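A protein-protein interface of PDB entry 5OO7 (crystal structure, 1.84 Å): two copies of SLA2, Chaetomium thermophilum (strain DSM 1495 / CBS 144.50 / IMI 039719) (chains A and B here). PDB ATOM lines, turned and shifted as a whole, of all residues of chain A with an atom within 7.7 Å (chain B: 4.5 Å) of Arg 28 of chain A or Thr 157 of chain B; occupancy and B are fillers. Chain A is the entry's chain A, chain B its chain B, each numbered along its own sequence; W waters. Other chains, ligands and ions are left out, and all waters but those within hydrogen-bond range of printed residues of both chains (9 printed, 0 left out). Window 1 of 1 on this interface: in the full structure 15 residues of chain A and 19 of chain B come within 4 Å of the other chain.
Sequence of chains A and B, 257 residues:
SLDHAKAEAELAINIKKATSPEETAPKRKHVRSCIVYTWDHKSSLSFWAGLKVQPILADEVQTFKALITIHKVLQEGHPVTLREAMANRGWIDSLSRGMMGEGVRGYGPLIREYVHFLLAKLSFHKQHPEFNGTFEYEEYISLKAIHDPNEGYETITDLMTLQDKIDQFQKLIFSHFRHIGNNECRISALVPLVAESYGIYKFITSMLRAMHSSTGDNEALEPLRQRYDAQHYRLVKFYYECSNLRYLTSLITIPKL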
ATOM      1  N   LYS A  17       1.661  -4.349   0.208  1.00  0.00           N
ATOM      2  CA  LYS A  17       2.634  -3.510  -0.502  1.00  0.00           C
ATOM      3  C   LYS A  17       1.984  -2.626  -1.575  1.00  0.00           C
ATOM      4  O   LYS A  17       2.413  -1.488  -1.781  1.00  0.00           O
ATOM      5  CB  LYS A  17       3.757  -4.370  -1.094  1.00  0.00           C
ATOM      6  CG  LYS A  17       4.642  -4.996  -0.021  1.00  0.00           C
ATOM      7  CD  LYS A  17       5.733  -5.876  -0.614  1.00  0.00           C
ATOM      8  CE  LYS A  17       6.622  -6.505   0.451  1.00  0.00           C
ATOM      9  NZ  LYS A  17       7.173  -5.528   1.430  1.00  0.00           N
ATOM     10  N   ALA A  18       0.948  -3.144  -2.237  1.00  0.00           N
ATOM     11  CA  ALA A  18       0.171  -2.365  -3.212  1.00  0.00           C
ATOM     12  C   ALA A  18      -0.596  -1.198  -2.580  1.00  0.00           C
ATOM     13  O   ALA A  18      -0.802  -0.175  -3.235  1.00  0.00           O
ATOM     14  CB  ALA A  18      -0.793  -3.270  -3.966  1.00  0.00           C
ATOM     15  N   ALA A  25       2.221   5.467  -7.114  1.00  0.00           N
ATOM     16  CA  ALA A  25       1.384   4.480  -7.790  1.00  0.00           C
ATOM     17  C   ALA A  25       1.480   3.177  -6.994  1.00  0.00           C
ATOM     18  O   ALA A  25       2.545   2.877  -6.444  1.00  0.00           O
ATOM     19  CB  ALA A  25       1.859   4.261  -9.217  1.00  0.00           C
ATOM     20  N   PRO A  26       0.370   2.415  -6.893  1.00  0.00           N
ATOM     21  CA  PRO A  26       0.471   1.090  -6.277  1.00  0.00           C
ATOM     22  C   PRO A  26       1.587   0.281  -6.938  1.00  0.00           C
ATOM     23  O   PRO A  26       1.606   0.175  -8.167  1.00  0.00           O
ATOM     24  CB  PRO A  26      -0.903   0.473  -6.560  1.00  0.00           C
ATOM     25  CG  PRO A  26      -1.822   1.640  -6.627  1.00  0.00           C
ATOM     26  CD  PRO A  26      -1.022   2.746  -7.254  1.00  0.00           C
ATOM     27  N   LYS A  27       2.530  -0.235  -6.145  1.00  0.00           N
ATOM     28  CA  LYS A  27       3.717  -0.890  -6.711  1.00  0.00           C
ATOM     29  C   LYS A  27       3.266  -1.971  -7.692  1.00  0.00           C
ATOM     30  O   LYS A  27       2.543  -2.901  -7.324  1.00  0.00           O
ATOM     31  CB  LYS A  27       4.655  -1.450  -5.630  1.00  0.00           C
ATOM     32  CG  LYS A  27       6.036  -1.824  -6.174  1.00  0.00           C
ATOM     33  CD  LYS A  27       7.153  -1.811  -5.126  1.00  0.00           C
ATOM     34  CE  LYS A  27       7.206  -3.097  -4.313  1.00  0.00           C
ATOM     35  NZ  LYS A  27       8.467  -3.308  -3.550  1.00  0.00           N
ATOM     36  N   ARG A  28       3.680  -1.808  -8.948  1.00  0.00           N
ATOM     37  CA  ARG A  28       3.023  -2.454 -10.088  1.00  0.00           C
ATOM     38  C   ARG A  28       3.084  -3.983 -10.091  1.00  0.00           C
ATOM     39  O   ARG A  28       2.099  -4.634 -10.441  1.00  0.00           O
ATOM     40  CB  ARG A  28       3.585  -1.907 -11.403  1.00  0.00           C
ATOM     41  CG  ARG A  28       3.240  -0.445 -11.653  1.00  0.00           C
ATOM     42  CD  ARG A  28       4.029   0.104 -12.827  1.00  0.00           C
ATOM     43  NE  ARG A  28       3.697  -0.592 -14.070  1.00  0.00           N
ATOM     44  CZ  ARG A  28       4.345  -0.453 -15.227  1.00  0.00           C
ATOM     45  NH1 ARG A  28       5.389   0.369 -15.338  1.00  0.00           N
ATOM     46  NH2 ARG A  28       3.938  -1.145 -16.288  1.00  0.00           N
ATOM     47  N   LYS A  29       4.224  -4.547  -9.700  1.00  0.00           N
ATOM     48  CA  LYS A  29       4.381  -6.008  -9.658  1.00  0.00           C
ATOM     49  C   LYS A  29       3.442  -6.686  -8.651  1.00  0.00           C
ATOM     50  O   LYS A  29       3.039  -7.832  -8.856  1.00  0.00           O
ATOM     51  CB  LYS A  29       5.842  -6.404  -9.386  1.00  0.00           C
ATOM     52  CG  LYS A  29       6.347  -6.134  -7.974  1.00  0.00           C
ATOM     53  CD  LYS A  29       7.814  -6.506  -7.850  1.00  0.00           C
ATOM     54  CE  LYS A  29       8.260  -6.525  -6.398  1.00  0.00           C
ATOM     55  NZ  LYS A  29       9.728  -6.733  -6.278  1.00  0.00           N
ATOM     56  N   HIS A  30       3.096  -5.978  -7.575  1.00  0.00           N
ATOM     57  CA  HIS A  30       2.164  -6.497  -6.569  1.00  0.00           C
ATOM     58  C   HIS A  30       0.701  -6.406  -7.000  1.00  0.00           C
ATOM     59  O   HIS A  30      -0.089  -7.287  -6.660  1.00  0.00           O
ATOM     60  CB  HIS A  30       2.372  -5.799  -5.231  1.00  0.00           C
ATOM     61  CG  HIS A  30       3.717  -6.061  -4.636  1.00  0.00           C
ATOM     62  ND1 HIS A  30       4.091  -7.295  -4.152  1.00  0.00           N
ATOM     63  CD2 HIS A  30       4.787  -5.252  -4.473  1.00  0.00           C
ATOM     64  CE1 HIS A  30       5.333  -7.232  -3.707  1.00  0.00           C
ATOM     65  NE2 HIS A  30       5.778  -6.002  -3.887  1.00  0.00           N
ATOM     66  N   VAL A  31       0.345  -5.353  -7.740  1.00  0.00           N
ATOM     67  CA  VAL A  31      -0.983  -5.267  -8.365  1.00  0.00           C
ATOM     68  C   VAL A  31      -1.113  -6.388  -9.398  1.00  0.00           C
ATOM     69  O   VAL A  31      -2.147  -7.050  -9.475  1.00  0.00           O
ATOM     70  CB  VAL A  31      -1.244  -3.904  -9.054  1.00  0.00           C
ATOM     71  CG1 VAL A  31      -2.605  -3.904  -9.754  1.00  0.00           C
ATOM     72  CG2 VAL A  31      -1.173  -2.767  -8.044  1.00  0.00           C
ATOM     73  N   ARG A  32      -0.054  -6.586 -10.182  1.00  0.00           N
ATOM     74  CA  ARG A  32       0.006  -7.677 -11.153  1.00  0.00           C
ATOM     75  C   ARG A  32      -0.135  -9.043 -10.477  1.00  0.00           C
ATOM     76  O   ARG A  32      -0.843  -9.908 -10.989  1.00  0.00           O
ATOM     77  CB  ARG A  32       1.313  -7.610 -11.958  1.00  0.00           C
ATOM     78  CG  ARG A  32       1.467  -8.653 -13.064  1.00  0.00           C
ATOM     79  CD  ARG A  32       0.284  -8.691 -14.023  1.00  0.00           C
ATOM     80  NE  ARG A  32      -0.031  -7.366 -14.556  1.00  0.00           N
ATOM     81  CZ  ARG A  32      -1.104  -7.068 -15.290  1.00  0.00           C
ATOM     82  NH1 ARG A  32      -2.004  -7.999 -15.613  1.00  0.00           N
ATOM     83  NH2 ARG A  32      -1.271  -5.820 -15.716  1.00  0.00           N
ATOM     84  N   SER A  33       0.528  -9.224  -9.334  1.00  0.00           N
ATOM     85  CA  SER A  33       0.392 -10.451  -8.538  1.00  0.00           C
ATOM     86  C   SER A  33      -1.052 -10.701  -8.091  1.00  0.00           C
ATOM     87  O   SER A  33      -1.511 -11.847  -8.106  1.00  0.00           O
ATOM     88  CB  SER A  33       1.306 -10.417  -7.311  1.00  0.00           C
ATOM     89  OG  SER A  33       2.661 -10.266  -7.690  1.00  0.00           O
ATOM     90  N   CYS A  34      -1.759  -9.636  -7.704  1.00  0.00           N
ATOM     91  CA  CYS A  34      -3.185  -9.728  -7.357  1.00  0.00           C
ATOM     92  C   CYS A  34      -4.026 -10.155  -8.565  1.00  0.00           C
ATOM     93  O   CYS A  34      -4.906 -11.007  -8.435  1.00  0.00           O
ATOM     94  CB  CYS A  34      -3.721  -8.401  -6.797  1.00  0.00           C
ATOM     95  SG  CYS A  34      -3.037  -7.885  -5.200  1.00  0.00           S
ATOM     96  N   ILE A  35      -3.745  -9.564  -9.731  1.00  0.00           N
ATOM     97  CA  ILE A  35      -4.450  -9.906 -10.977  1.00  0.00           C
ATOM     98  C   ILE A  35      -4.177 -11.366 -11.359  1.00  0.00           C
ATOM     99  O   ILE A  35      -5.112 -12.124 -11.618  1.00  0.00           O
ATOM    100  CB  ILE A  35      -4.062  -8.961 -12.148  1.00  0.00           C
ATOM    101  CG1 ILE A  35      -4.550  -7.530 -11.877  1.00  0.00           C
ATOM    102  CG2 ILE A  35      -4.633  -9.460 -13.478  1.00  0.00           C
ATOM    103  CD1 ILE A  35      -3.820  -6.465 -12.672  1.00  0.00           C
ATOM    104  N   LYS A  72      -8.062  -1.988 -11.095  1.00  0.00           N
ATOM    105  CA  LYS A  72      -7.191  -2.778 -11.971  1.00  0.00           C
ATOM    106  C   LYS A  72      -7.506  -4.281 -11.927  1.00  0.00           C
ATOM    107  O   LYS A  72      -7.478  -4.948 -12.962  1.00  0.00           O
ATOM    108  CB  LYS A  72      -5.719  -2.520 -11.632  1.00  0.00           C
ATOM    109  CG  LYS A  72      -5.261  -1.110 -11.978  1.00  0.00           C
ATOM    110  CD  LYS A  72      -3.926  -0.772 -11.334  1.00  0.00           C
ATOM    111  CE  LYS A  72      -3.385   0.558 -11.828  1.00  0.00           C
ATOM    112  NZ  LYS A  72      -2.725   0.437 -13.156  1.00  0.00           N
ATOM    113  N   GLU A  76      -8.681  -6.458 -15.187  1.00  0.00           N
ATOM    114  CA  GLU A  76      -7.773  -7.460 -15.754  1.00  0.00           C
ATOM    115  C   GLU A  76      -7.832  -8.853 -15.131  1.00  0.00           C
ATOM    116  O   GLU A  76      -7.236  -9.788 -15.672  1.00  0.00           O
ATOM    117  CB  GLU A  76      -6.340  -6.939 -15.671  1.00  0.00           C
ATOM    118  CG  GLU A  76      -6.113  -5.666 -16.467  1.00  0.00           C
ATOM    119  CD  GLU A  76      -4.664  -5.237 -16.466  1.00  0.00           C
ATOM    120  OE1 GLU A  76      -3.809  -6.024 -16.924  1.00  0.00           O
ATOM    121  OE2 GLU A  76      -4.375  -4.115 -16.005  1.00  0.00           O
ATOM    122  N   SER A 188      -1.654   7.639 -11.582  1.00  0.00           N
ATOM    123  CA  SER A 188      -1.814   6.183 -11.699  1.00  0.00           C
ATOM    124  C   SER A 188      -3.281   5.728 -11.720  1.00  0.00           C
ATOM    125  O   SER A 188      -3.565   4.629 -12.187  1.00  0.00           O
ATOM    126  CB  SER A 188      -1.051   5.450 -10.589  1.00  0.00           C
ATOM    127  OG  SER A 188      -1.644   5.661  -9.321  1.00  0.00           O
ATOM    128  N   TYR A 247       4.474  10.137 -16.966  1.00  0.00           N
ATOM    129  CA  TYR A 247       4.249   8.847 -16.300  1.00  0.00           C
ATOM    130  C   TYR A 247       3.141   8.048 -16.993  1.00  0.00           C
ATOM    131  O   TYR A 247       3.282   6.841 -17.198  1.00  0.00           O
ATOM    132  CB  TYR A 247       3.910   9.040 -14.818  1.00  0.00           C
ATOM    133  CG  TYR A 247       3.735   7.736 -14.064  1.00  0.00           C
ATOM    134  CD1 TYR A 247       4.828   6.914 -13.792  1.00  0.00           C
ATOM    135  CD2 TYR A 247       2.474   7.320 -13.633  1.00  0.00           C
ATOM    136  CE1 TYR A 247       4.672   5.716 -13.108  1.00  0.00           C
ATOM    137  CE2 TYR A 247       2.308   6.124 -12.947  1.00  0.00           C
ATOM    138  CZ  TYR A 247       3.407   5.327 -12.686  1.00  0.00           C
ATOM    139  OH  TYR A 247       3.242   4.144 -12.009  1.00  0.00           O
ATOM    140  N   THR A 249       1.911   8.419 -20.222  1.00  0.00           N
ATOM    141  CA  THR A 249       2.292   8.046 -21.592  1.00  0.00           C
ATOM    142  C   THR A 249       3.367   6.950 -21.657  1.00  0.00           C
ATOM    143  O   THR A 249       3.475   6.256 -22.668  1.00  0.00           O
ATOM    144  CB  THR A 249       2.759   9.268 -22.409  1.00  0.00           C
ATOM    145  OG1 THR A 249       3.800   9.951 -21.707  1.00  0.00           O
ATOM    146  CG2 THR A 249       1.600  10.222 -22.649  1.00  0.00           C
ATOM    147  N   SER A 250       4.157   6.802 -20.594  1.00  0.00           N
ATOM    148  CA  SER A 250       5.112   5.693 -20.475  1.00  0.00           C
ATOM    149  C   SER A 250       4.443   4.332 -20.227  1.00  0.00           C
ATOM    150  O   SER A 250       5.018   3.295 -20.562  1.00  0.00           O
ATOM    151  CB  SER A 250       6.117   5.977 -19.356  1.00  0.00           C
ATOM    152  OG  SER A 250       6.884   7.129 -19.650  1.00  0.00           O
ATOM    153  N   LEU A 251       3.247   4.349 -19.636  1.00  0.00           N
ATOM    154  CA  LEU A 251       2.499   3.130 -19.283  1.00  0.00           C
ATOM    155  C   LEU A 251       1.448   2.725 -20.321  1.00  0.00           C
ATOM    156  O   LEU A 251       1.194   1.533 -20.499  1.00  0.00           O
ATOM    157  CB  LEU A 251       1.825   3.295 -17.909  1.00  0.00           C
ATOM    158  CG  LEU A 251       2.649   2.971 -16.654  1.00  0.00           C
ATOM    159  CD1 LEU A 251       4.099   3.426 -16.747  1.00  0.00           C
ATOM    160  CD2 LEU A 251       1.978   3.577 -15.428  1.00  0.00           C
ATOM    161  N   ILE A 252       0.826   3.704 -20.980  1.00  0.00           N
ATOM    162  CA  ILE A 252      -0.227   3.439 -21.967  1.00  0.00           C
ATOM    163  C   ILE A 252      -0.126   4.355 -23.183  1.00  0.00           C
ATOM    164  O   ILE A 252       0.354   5.487 -23.083  1.00  0.00           O
ATOM    165  CB  ILE A 252      -1.645   3.577 -21.355  1.00  0.00           C
ATOM    166  CG1 ILE A 252      -1.821   4.930 -20.649  1.00  0.00           C
ATOM    167  CG2 ILE A 252      -1.923   2.438 -20.384  1.00  0.00           C
ATOM    168  CD1 ILE A 252      -3.254   5.245 -20.289  1.00  0.00           C
ATOM    169  N   THR A 253      -0.581   3.843 -24.325  1.00  0.00           N
ATOM    170  CA  THR A 253      -0.718   4.628 -25.542  1.00  0.00           C
ATOM    171  C   THR A 253      -2.065   5.335 -25.491  1.00  0.00           C
ATOM    172  O   THR A 253      -3.107   4.686 -25.356  1.00  0.00           O
ATOM    173  CB  THR A 253      -0.652   3.735 -26.798  1.00  0.00           C
ATOM    174  OG1 THR A 253       0.616   3.072 -26.838  1.00  0.00           O
ATOM    175  CG2 THR A 253      -0.829   4.557 -28.077  1.00  0.00           C
ATOM    176  N   GLN B 127      12.784   3.585 -15.552  1.00  0.00           N
ATOM    177  CA  GLN B 127      11.919   2.574 -14.908  1.00  0.00           C
ATOM    178  C   GLN B 127      12.562   1.183 -14.869  1.00  0.00           C
ATOM    179  O   GLN B 127      12.391   0.447 -13.895  1.00  0.00           O
ATOM    180  CB  GLN B 127      10.570   2.456 -15.637  1.00  0.00           C
ATOM    181  CG  GLN B 127       9.646   3.660 -15.508  1.00  0.00           C
ATOM    182  CD  GLN B 127       8.381   3.537 -16.347  1.00  0.00           C
ATOM    183  OE1 GLN B 127       8.387   2.954 -17.437  1.00  0.00           O
ATOM    184  NE2 GLN B 127       7.285   4.100 -15.845  1.00  0.00           N
ATOM    185  N   TYR B 153       5.553  -9.014 -17.018  1.00  0.00           N
ATOM    186  CA  TYR B 153       4.282  -8.568 -17.609  1.00  0.00           C
ATOM    187  C   TYR B 153       4.264  -7.043 -17.759  1.00  0.00           C
ATOM    188  O   TYR B 153       3.996  -6.526 -18.845  1.00  0.00           O
ATOM    189  CB  TYR B 153       3.085  -9.027 -16.756  1.00  0.00           C
ATOM    190  CG  TYR B 153       1.742  -8.952 -17.465  1.00  0.00           C
ATOM    191  CD1 TYR B 153       1.059 -10.113 -17.837  1.00  0.00           C
ATOM    192  CD2 TYR B 153       1.145  -7.720 -17.760  1.00  0.00           C
ATOM    193  CE1 TYR B 153      -0.170 -10.047 -18.485  1.00  0.00           C
ATOM    194  CE2 TYR B 153      -0.078  -7.647 -18.407  1.00  0.00           C
ATOM    195  CZ  TYR B 153      -0.734  -8.808 -18.765  1.00  0.00           C
ATOM    196  OH  TYR B 153      -1.945  -8.721 -19.406  1.00  0.00           O
ATOM    197  N   GLU B 154       4.560  -6.345 -16.666  1.00  0.00           N
ATOM    198  CA  GLU B 154       4.547  -4.876 -16.638  1.00  0.00           C
ATOM    199  C   GLU B 154       5.608  -4.272 -17.563  1.00  0.00           C
ATOM    200  O   GLU B 154       5.365  -3.248 -18.203  1.00  0.00           O
ATOM    201  CB  GLU B 154       4.750  -4.358 -15.208  1.00  0.00           C
ATOM    202  CG  GLU B 154       3.642  -4.716 -14.224  1.00  0.00           C
ATOM    203  CD  GLU B 154       2.280  -4.159 -14.602  1.00  0.00           C
ATOM    204  OE1 GLU B 154       2.204  -3.015 -15.102  1.00  0.00           O
ATOM    205  OE2 GLU B 154       1.276  -4.874 -14.387  1.00  0.00           O
ATOM    206  N   THR B 155       6.772  -4.917 -17.626  1.00  0.00           N
ATOM    207  CA  THR B 155       7.854  -4.507 -18.523  1.00  0.00           C
ATOM    208  C   THR B 155       7.470  -4.630 -20.005  1.00  0.00           C
ATOM    209  O   THR B 155       7.793  -3.743 -20.799  1.00  0.00           O
ATOM    210  CB  THR B 155       9.132  -5.327 -18.246  1.00  0.00           C
ATOM    211  OG1 THR B 155       9.522  -5.149 -16.879  1.00  0.00           O
ATOM    212  CG2 THR B 155      10.278  -4.892 -19.145  1.00  0.00           C
ATOM    213  N   ILE B 156       6.795  -5.721 -20.366  1.00  0.00           N
ATOM    214  CA  ILE B 156       6.336  -5.935 -21.749  1.00  0.00           C
ATOM    215  C   ILE B 156       5.325  -4.867 -22.182  1.00  0.00           C
ATOM    216  O   ILE B 156       5.428  -4.344 -23.292  1.00  0.00           O
ATOM    217  CB  ILE B 156       5.751  -7.359 -21.952  1.00  0.00           C
ATOM    218  CG1 ILE B 156       6.879  -8.399 -21.909  1.00  0.00           C
ATOM    219  CG2 ILE B 156       5.003  -7.477 -23.284  1.00  0.00           C
ATOM    220  CD1 ILE B 156       6.406  -9.807 -21.621  1.00  0.00           C
ATOM    221  N   THR B 157       4.362  -4.546 -21.316  1.00  0.00           N
ATOM    222  CA  THR B 157       3.369  -3.507 -21.631  1.00  0.00           C
ATOM    223  C   THR B 157       4.021  -2.128 -21.818  1.00  0.00           C
ATOM    224  O   THR B 157       3.590  -1.359 -22.679  1.00  0.00           O
ATOM    225  CB  THR B 157       2.239  -3.420 -20.578  1.00  0.00           C
ATOM    226  OG1 THR B 157       2.794  -3.173 -19.281  1.00  0.00           O
ATOM    227  CG2 THR B 157       1.425  -4.711 -20.548  1.00  0.00           C
ATOM    228  N   ASP B 158       5.061  -1.832 -21.034  1.00  0.00           N
ATOM    229  CA  ASP B 158       5.859  -0.610 -21.230  1.00  0.00           C
ATOM    230  C   ASP B 158       6.582  -0.615 -22.581  1.00  0.00           C
ATOM    231  O   ASP B 158       6.578   0.393 -23.291  1.00  0.00           O
ATOM    232  CB  ASP B 158       6.883  -0.418 -20.100  1.00  0.00           C
ATOM    233  CG  ASP B 158       6.241  -0.086 -18.760  1.00  0.00           C
ATOM    234  OD1 ASP B 158       4.994  -0.049 -18.657  1.00  0.00           O
ATOM    235  OD2 ASP B 158       6.995   0.136 -17.787  1.00  0.00           O
ATOM    236  N   LEU B 159       7.197  -1.747 -22.925  1.00  0.00           N
ATOM    237  CA  LEU B 159       7.861  -1.918 -24.227  1.00  0.00           C
ATOM    238  C   LEU B 159       6.897  -1.820 -25.411  1.00  0.00           C
ATOM    239  O   LEU B 159       7.242  -1.238 -26.443  1.00  0.00           O
ATOM    240  CB  LEU B 159       8.606  -3.257 -24.289  1.00  0.00           C
ATOM    241  CG  LEU B 159       9.891  -3.347 -23.462  1.00  0.00           C
ATOM    242  CD1 LEU B 159      10.319  -4.793 -23.298  1.00  0.00           C
ATOM    243  CD2 LEU B 159      11.009  -2.527 -24.091  1.00  0.00           C
ATOM    244  N   MET B 160       5.704  -2.398 -25.263  1.00  0.00           N
ATOM    245  CA  MET B 160       4.658  -2.312 -26.295  1.00  0.00           C
ATOM    246  C   MET B 160       4.175  -0.875 -26.517  1.00  0.00           C
ATOM    247  O   MET B 160       3.855  -0.491 -27.646  1.00  0.00           O
ATOM    248  CB  MET B 160       3.471  -3.215 -25.943  1.00  0.00           C
ATOM    249  CG  MET B 160       3.756  -4.700 -26.106  1.00  0.00           C
ATOM    250  SD  MET B 160       2.412  -5.731 -25.495  1.00  0.00           S
ATOM    251  CE  MET B 160       2.924  -7.342 -26.085  1.00  0.00           C
ATOM    252  N   THR B 161       4.120  -0.091 -25.442  1.00  0.00           N
ATOM    253  CA  THR B 161       3.795   1.335 -25.527  1.00  0.00           C
ATOM    254  C   THR B 161       4.893   2.117 -26.267  1.00  0.00           C
ATOM    255  O   THR B 161       4.591   3.027 -27.041  1.00  0.00           O
ATOM    256  CB  THR B 161       3.549   1.927 -24.121  1.00  0.00           C
ATOM    257  OG1 THR B 161       2.485   1.206 -23.485  1.00  0.00           O
ATOM    258  CG2 THR B 161       3.179   3.403 -24.189  1.00  0.00           C
ATOM    259  N   LEU B 224      -1.465  -9.872 -23.674  1.00  0.00           N
ATOM    260  CA  LEU B 224      -0.119  -9.687 -24.224  1.00  0.00           C
ATOM    261  C   LEU B 224       0.054 -10.402 -25.564  1.00  0.00           C
ATOM    262  O   LEU B 224       0.652  -9.840 -26.480  1.00  0.00           O
ATOM    263  CB  LEU B 224       0.959 -10.157 -23.237  1.00  0.00           C
ATOM    264  CG  LEU B 224       1.041  -9.449 -21.879  1.00  0.00           C
ATOM    265  CD1 LEU B 224       2.284  -9.912 -21.134  1.00  0.00           C
ATOM    266  CD2 LEU B 224       1.036  -7.933 -22.019  1.00  0.00           C
ATOM    267  N   ARG B 227      -1.909  -8.330 -28.242  1.00  0.00           N
ATOM    268  CA  ARG B 227      -1.168  -7.103 -28.547  1.00  0.00           C
ATOM    269  C   ARG B 227       0.166  -7.396 -29.242  1.00  0.00           C
ATOM    270  O   ARG B 227       0.579  -6.639 -30.121  1.00  0.00           O
ATOM    271  CB  ARG B 227      -0.939  -6.273 -27.278  1.00  0.00           C
ATOM    272  CG  ARG B 227      -0.498  -4.843 -27.550  1.00  0.00           C
ATOM    273  CD  ARG B 227      -0.628  -3.967 -26.314  1.00  0.00           C
ATOM    274  NE  ARG B 227      -0.109  -2.618 -26.546  1.00  0.00           N
ATOM    275  CZ  ARG B 227       0.193  -1.727 -25.597  1.00  0.00           C
ATOM    276  NH1 ARG B 227       0.044  -2.010 -24.301  1.00  0.00           N
ATOM    277  NH2 ARG B 227       0.658  -0.529 -25.949  1.00  0.00           N
HETATM  278  O   HOH W   1      -3.096  -6.319 -19.734  1.00  0.00           O
HETATM  279  O   HOH W   2      -0.201  -0.281 -22.081  1.00  0.00           O
HETATM  280  O   HOH W   3       2.408   5.308 -26.984  1.00  0.00           O
HETATM  281  O   HOH W   4       0.654  -4.169 -17.513  1.00  0.00           O
HETATM  282  O   HOH W   5       6.641   2.347 -13.772  1.00  0.00           O
HETATM  283  O   HOH W   6       6.993   2.892 -22.398  1.00  0.00           O
HETATM  284  O   HOH W   7      -1.413   0.993 -24.201  1.00  0.00           O
HETATM  285  O   HOH W   8       8.288   3.281 -20.132  1.00  0.00           O
HETATM  286  O   HOH W   9       2.308  -0.418 -19.017  1.00  0.00           O
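Hydrophobic or aromatic side chains of chain B that line the printed part of chain A: Tyr 153. Of the 22 printed residues of chain A, 7 touch a printed residue of chain B. Printed residues of chain A that touch a printed residue of chain B: Arg 28, Arg 32, Thr 249, Ser 250, Leu 251, Ile 252 and Thr 253. Hydrophobic or aromatic side chains of chain A within 4 Å of the printed part of chain B: Leu 251. Among the printed residues, Asp or Glu carboxylates within 4 Å of a Lys or Arg side-chain nitrogen of the other chain: Arg 28 of chain A with Glu 154 of chain B, Arg 28 of chain A with Asp 158 of chain B and Arg 32 of chain A with Glu 154 of chain B.
Ile 35 of chain A touches none of the printed residues of chain B. Printed residues of chain A within 4 Å of Gln 127 of chain B: Leu 251. Of the printed residues of chain A, Tyr 153 of chain B touches Arg 32. Ile 156 of chain B touches none of the printed residues of chain A. Thr 157 of chain B touches one residue of chain A. The nearest residue of chain B that does not touch Arg 28 of chain A is Gln 127 of chain B (4.2 Å). The nearest residue of chain A that does not touch Thr 157 of chain B is Leu 251 of chain A (4.3 Å).
NH2 of Arg 28 of chain A lies within salt-bridge range of OE1 of Glu 154 of chain B (2.8 Å). The side-chain carboxylate (OD1) of Asp 158 of chain B is in salt-bridge range of the guanidinium group (NH2) of Arg 28 of chain A. The guanidinium group (NE) of Arg 32 of chain A lies within salt-bridge range of the side-chain carboxylate (OE2) of Glu 154 of chain B, at 2.8 Å. The side-chain hydroxyl (OG1) of Thr 161 of chain B lies within hydrogen-bond range of the backbone carbonyl oxygen (O) of Leu 251 of chain A.
The backbone carbonyl oxygen (O) of Glu 154 of chain B is in hydrogen-bond range of the side-chain hydroxyl (OG1) of Thr 157 of chain B (2.8 Å). OD2 of Asp 158 of chain B lies close to OE1 of Gln 127 of chain B (3.2 Å). NH2 of Arg 32 of chain A is in salt-bridge range of OE1 of Glu 76 of chain A. O of Thr 157 of chain B sits at hydrogen-bond distance from OG1 of Thr 161 of chain B.
Among the printed residues, pairs that only touch across the chains: Arg 28 of chain A with Thr 157 of chain B (3.8 Å), Arg 32 of chain A with Tyr 153 of chain B (3.3 Å), Thr 249 of chain A with Thr 161 of chain B (3.2 Å), Ser 250 of chain A with Asp 158 of chain B (3.8 Å), Leu 251 of chain A with Gln 127 of chain B (3.4 Å), Ile 252 of chain A with Thr 161 of chain B (3.6 Å), Thr 253 of chain A with Thr 161 of chain B (3.7 Å) and Thr 253 of chain A with Arg 227 of chain B (3.7 Å).
No position is printed for both chains. Of the 12 pairs that touch across the chains among the printed residues, none has its exchanged pair printed and touching as well.
Water W1 lies within hydrogen-bond range of OH of Tyr 153 of chain B and OE1 of Glu 76 of chain A. Water W6 lies within hydrogen-bond range of the backbone carbonyl oxygen of Asp 158 of chain B (2.7 Å) and the backbone carbonyl oxygen of Ser 250 of chain A (2.7 Å). Water W9 lies within hydrogen-bond range of O of Leu 251 of chain A (2.7 Å), OD1 of Asp 158 of chain B (2.7 Å), OG1 of Thr 157 of chain B (2.8 Å) and NH2 of Arg 28 of chain A (3.3 Å). Water W2 lies within hydrogen-bond range of O of Leu 251 of chain A (2.8 Å), NH1 of Arg 227 of chain B (2.8 Å) and OG1 of Thr 161 of chain B (3.4 Å). Water W5 bridges the side-chain amide nitrogen (NE2) of Gln 127 of chain B (2.8 Å) and the guanidinium group (NH1) of Arg 28 of chain A (2.8 Å). Water W3 bridges the side-chain hydroxyl of Thr 253 of chain A (2.9 Å) and the backbone carbonyl oxygen of Thr 161 of chain B (3.2 Å).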
